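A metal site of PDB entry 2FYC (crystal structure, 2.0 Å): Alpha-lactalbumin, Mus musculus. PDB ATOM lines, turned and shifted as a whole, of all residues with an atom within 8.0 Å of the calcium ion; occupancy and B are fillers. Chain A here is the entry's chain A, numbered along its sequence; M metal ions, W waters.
Within 4 Å of the calcium ion: Lys 79, Asp 82, Glu 84, Asp 87 and Asp 88.
The nearest printed residue that does not touch the calcium ion is Leu 80 (4.2 Å).
O of Glu 84 binds the calcium ion (2.2 Å).
The calcium ion is bound by O of Lys 79.
The calcium ion is bound by the side-chain carboxylate (OD1) of Asp 87 (2.4 Å).
OD2 of Asp 88 binds the calcium ion (2.5 Å).
Water W2 is bound to the calcium ion, at 2.5 Å.
The calcium ion is bound by water W1 (2.5 Å).
The side-chain carboxylate (OD1) of Asp 82 is bound to the calcium ion (2.5 Å).
The calcium ion has seven donor atoms within binding distance.
Water W1 bridges OD2 of Asp 87 and OD2 of Asp 82.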
ATOM      1  N   THR A  38      -3.819  16.187 -17.804  1.00  0.00           N
ATOM      2  CA  THR A  38      -4.740  17.086 -17.104  1.00  0.00           C
ATOM      3  C   THR A  38      -6.142  16.473 -16.933  1.00  0.00           C
ATOM      4  O   THR A  38      -6.949  16.990 -16.194  1.00  0.00           O
ATOM      5  CB  THR A  38      -4.874  18.441 -17.830  1.00  0.00           C
ATOM      6  OG1 THR A  38      -5.443  18.251 -19.135  1.00  0.00           O
ATOM      7  CG2 THR A  38      -3.498  19.087 -17.990  1.00  0.00           C
ATOM      8  N   GLY A  51      -7.265  15.318 -12.263  1.00  0.00           N
ATOM      9  CA  GLY A  51      -6.265  16.135 -12.917  1.00  0.00           C
ATOM     10  C   GLY A  51      -4.800  15.899 -12.686  1.00  0.00           C
ATOM     11  O   GLY A  51      -4.377  14.885 -12.109  1.00  0.00           O
ATOM     12  N   ILE A  75     -14.168  24.207  -4.918  1.00  0.00           N
ATOM     13  CA  ILE A  75     -14.232  24.077  -6.365  1.00  0.00           C
ATOM     14  C   ILE A  75     -14.824  22.751  -6.849  1.00  0.00           C
ATOM     15  O   ILE A  75     -14.737  21.727  -6.169  1.00  0.00           O
ATOM     16  CB  ILE A  75     -12.776  24.283  -6.919  1.00  0.00           C
ATOM     17  CG1 ILE A  75     -12.805  24.653  -8.386  1.00  0.00           C
ATOM     18  CG2 ILE A  75     -11.913  23.011  -6.728  1.00  0.00           C
ATOM     19  CD1 ILE A  75     -11.424  24.840  -8.938  1.00  0.00           C
ATOM     20  N   SER A  76     -15.456  22.785  -8.029  1.00  0.00           N
ATOM     21  CA  SER A  76     -15.997  21.562  -8.607  1.00  0.00           C
ATOM     22  C   SER A  76     -14.815  20.752  -9.096  1.00  0.00           C
ATOM     23  O   SER A  76     -13.887  21.311  -9.695  1.00  0.00           O
ATOM     24  CB  SER A  76     -16.887  21.854  -9.825  1.00  0.00           C
ATOM     25  OG  SER A  76     -17.081  20.641 -10.567  1.00  0.00           O
ATOM     26  N   CYS A  77     -14.816  19.462  -8.844  1.00  0.00           N
ATOM     27  CA  CYS A  77     -13.695  18.671  -9.329  1.00  0.00           C
ATOM     28  C   CYS A  77     -13.555  18.733 -10.865  1.00  0.00           C
ATOM     29  O   CYS A  77     -12.466  18.488 -11.397  1.00  0.00           O
ATOM     30  CB  CYS A  77     -13.844  17.214  -8.882  1.00  0.00           C
ATOM     31  SG  CYS A  77     -13.940  16.950  -7.064  1.00  0.00           S
ATOM     32  N   ASP A  78     -14.622  19.084 -11.589  1.00  0.00           N
ATOM     33  CA  ASP A  78     -14.492  19.156 -13.061  1.00  0.00           C
ATOM     34  C   ASP A  78     -13.576  20.289 -13.509  1.00  0.00           C
ATOM     35  O   ASP A  78     -13.008  20.233 -14.599  1.00  0.00           O
ATOM     36  CB  ASP A  78     -15.863  19.320 -13.746  1.00  0.00           C
ATOM     37  CG  ASP A  78     -16.762  18.131 -13.530  1.00  0.00           C
ATOM     38  OD1 ASP A  78     -16.249  16.989 -13.543  1.00  0.00           O
ATOM     39  OD2 ASP A  78     -17.982  18.348 -13.345  1.00  0.00           O
ATOM     40  N   LYS A  79     -13.438  21.314 -12.675  1.00  0.00           N
ATOM     41  CA  LYS A  79     -12.537  22.413 -12.999  1.00  0.00           C
ATOM     42  C   LYS A  79     -11.068  21.951 -12.945  1.00  0.00           C
ATOM     43  O   LYS A  79     -10.147  22.681 -13.333  1.00  0.00           O
ATOM     44  CB  LYS A  79     -12.767  23.570 -12.024  1.00  0.00           C
ATOM     45  CG  LYS A  79     -14.117  24.302 -12.186  1.00  0.00           C
ATOM     46  CD  LYS A  79     -14.092  25.091 -13.497  1.00  0.00           C
ATOM     47  CE  LYS A  79     -15.328  25.989 -13.665  1.00  0.00           C
ATOM     48  NZ  LYS A  79     -14.983  27.117 -14.593  1.00  0.00           N
ATOM     49  N   LEU A  80     -10.860  20.712 -12.472  1.00  0.00           N
ATOM     50  CA  LEU A  80      -9.530  20.171 -12.345  1.00  0.00           C
ATOM     51  C   LEU A  80      -9.235  19.218 -13.487  1.00  0.00           C
ATOM     52  O   LEU A  80      -8.218  18.532 -13.457  1.00  0.00           O
ATOM     53  CB  LEU A  80      -9.370  19.451 -10.990  1.00  0.00           C
ATOM     54  CG  LEU A  80      -9.701  20.330  -9.780  1.00  0.00           C
ATOM     55  CD1 LEU A  80      -9.614  19.536  -8.481  1.00  0.00           C
ATOM     56  CD2 LEU A  80      -8.758  21.506  -9.755  1.00  0.00           C
ATOM     57  N   LEU A  81     -10.127  19.173 -14.479  1.00  0.00           N
ATOM     58  CA  LEU A  81      -9.950  18.292 -15.611  1.00  0.00           C
ATOM     59  C   LEU A  81      -9.792  19.035 -16.924  1.00  0.00           C
ATOM     60  O   LEU A  81     -10.079  18.484 -17.960  1.00  0.00           O
ATOM     61  CB  LEU A  81     -11.145  17.323 -15.745  1.00  0.00           C
ATOM     62  CG  LEU A  81     -11.365  16.311 -14.610  1.00  0.00           C
ATOM     63  CD1 LEU A  81     -12.530  15.371 -14.920  1.00  0.00           C
ATOM     64  CD2 LEU A  81     -10.082  15.514 -14.446  1.00  0.00           C
ATOM     65  N   ASP A  82      -9.324  20.270 -16.883  1.00  0.00           N
ATOM     66  CA  ASP A  82      -9.135  21.005 -18.129  1.00  0.00           C
ATOM     67  C   ASP A  82      -7.688  21.472 -18.196  1.00  0.00           C
ATOM     68  O   ASP A  82      -6.871  21.123 -17.331  1.00  0.00           O
ATOM     69  CB  ASP A  82     -10.104  22.188 -18.205  1.00  0.00           C
ATOM     70  CG  ASP A  82     -10.003  23.110 -16.999  1.00  0.00           C
ATOM     71  OD1 ASP A  82      -8.857  23.381 -16.580  1.00  0.00           O
ATOM     72  OD2 ASP A  82     -11.038  23.576 -16.476  1.00  0.00           O
ATOM     73  N   ASP A  83      -7.367  22.276 -19.202  1.00  0.00           N
ATOM     74  CA  ASP A  83      -6.001  22.742 -19.426  1.00  0.00           C
ATOM     75  C   ASP A  83      -5.605  24.083 -18.834  1.00  0.00           C
ATOM     76  O   ASP A  83      -4.582  24.631 -19.194  1.00  0.00           O
ATOM     77  CB  ASP A  83      -5.749  22.748 -20.928  1.00  0.00           C
ATOM     78  CG  ASP A  83      -5.627  21.336 -21.497  1.00  0.00           C
ATOM     79  OD1 ASP A  83      -5.790  20.364 -20.722  1.00  0.00           O
ATOM     80  OD2 ASP A  83      -5.357  21.221 -22.719  1.00  0.00           O
ATOM     81  N   GLU A  84      -6.398  24.583 -17.915  1.00  0.00           N
ATOM     82  CA  GLU A  84      -6.154  25.850 -17.255  1.00  0.00           C
ATOM     83  C   GLU A  84      -5.793  25.413 -15.857  1.00  0.00           C
ATOM     84  O   GLU A  84      -6.650  24.993 -15.059  1.00  0.00           O
ATOM     85  CB  GLU A  84      -7.423  26.703 -17.319  1.00  0.00           C
ATOM     86  CG  GLU A  84      -7.644  27.239 -18.760  1.00  0.00           C
ATOM     87  CD  GLU A  84      -9.074  27.653 -19.048  1.00  0.00           C
ATOM     88  OE1 GLU A  84      -9.596  28.569 -18.353  1.00  0.00           O
ATOM     89  OE2 GLU A  84      -9.655  27.072 -19.979  1.00  0.00           O
ATOM     90  N   LEU A  85      -4.506  25.508 -15.554  1.00  0.00           N
ATOM     91  CA  LEU A  85      -3.995  25.000 -14.298  1.00  0.00           C
ATOM     92  C   LEU A  85      -3.999  25.967 -13.133  1.00  0.00           C
ATOM     93  O   LEU A  85      -3.672  25.567 -12.014  1.00  0.00           O
ATOM     94  CB  LEU A  85      -2.578  24.472 -14.529  1.00  0.00           C
ATOM     95  CG  LEU A  85      -2.318  23.022 -14.952  1.00  0.00           C
ATOM     96  CD1 LEU A  85      -3.534  22.317 -15.539  1.00  0.00           C
ATOM     97  CD2 LEU A  85      -1.134  23.014 -15.893  1.00  0.00           C
ATOM     98  N   ASP A  86      -4.404  27.216 -13.365  1.00  0.00           N
ATOM     99  CA  ASP A  86      -4.411  28.181 -12.278  1.00  0.00           C
ATOM    100  C   ASP A  86      -5.258  27.703 -11.104  1.00  0.00           C
ATOM    101  O   ASP A  86      -4.783  27.747  -9.969  1.00  0.00           O
ATOM    102  CB  ASP A  86      -4.888  29.571 -12.733  1.00  0.00           C
ATOM    103  CG  ASP A  86      -3.850  30.316 -13.587  1.00  0.00           C
ATOM    104  OD1 ASP A  86      -3.724  29.992 -14.790  1.00  0.00           O
ATOM    105  OD2 ASP A  86      -3.181  31.250 -13.081  1.00  0.00           O
ATOM    106  N   ASP A  87      -6.493  27.244 -11.331  1.00  0.00           N
ATOM    107  CA  ASP A  87      -7.263  26.783 -10.182  1.00  0.00           C
ATOM    108  C   ASP A  87      -6.695  25.464  -9.588  1.00  0.00           C
ATOM    109  O   ASP A  87      -6.732  25.287  -8.368  1.00  0.00           O
ATOM    110  CB  ASP A  87      -8.781  26.674 -10.481  1.00  0.00           C
ATOM    111  CG  ASP A  87      -9.101  25.927 -11.784  1.00  0.00           C
ATOM    112  OD1 ASP A  87      -8.215  25.276 -12.378  1.00  0.00           O
ATOM    113  OD2 ASP A  87     -10.280  25.976 -12.202  1.00  0.00           O
ATOM    114  N   ASP A  88      -6.142  24.562 -10.420  1.00  0.00           N
ATOM    115  CA  ASP A  88      -5.536  23.334  -9.854  1.00  0.00           C
ATOM    116  C   ASP A  88      -4.380  23.702  -8.922  1.00  0.00           C
ATOM    117  O   ASP A  88      -4.237  23.115  -7.853  1.00  0.00           O
ATOM    118  CB  ASP A  88      -4.957  22.403 -10.932  1.00  0.00           C
ATOM    119  CG  ASP A  88      -5.954  22.083 -12.036  1.00  0.00           C
ATOM    120  OD1 ASP A  88      -6.112  20.895 -12.405  1.00  0.00           O
ATOM    121  OD2 ASP A  88      -6.572  23.044 -12.523  1.00  0.00           O
ATOM    122  N   ILE A  89      -3.587  24.681  -9.334  1.00  0.00           N
ATOM    123  CA  ILE A  89      -2.434  25.142  -8.563  1.00  0.00           C
ATOM    124  C   ILE A  89      -2.868  25.753  -7.226  1.00  0.00           C
ATOM    125  O   ILE A  89      -2.298  25.450  -6.191  1.00  0.00           O
ATOM    126  CB  ILE A  89      -1.592  26.153  -9.392  1.00  0.00           C
ATOM    127  CG1 ILE A  89      -0.938  25.408 -10.569  1.00  0.00           C
ATOM    128  CG2 ILE A  89      -0.534  26.834  -8.498  1.00  0.00           C
ATOM    129  CD1 ILE A  89      -0.366  26.333 -11.673  1.00  0.00           C
HETATM  130 CA    CA M   1      -8.255  23.742 -14.172  1.00  0.00          CA
HETATM  131  O   HOH W   1     -10.090  25.369 -14.685  1.00  0.00           O
HETATM  132  O   HOH W   2      -7.508  21.471 -14.753  1.00  0.00           O
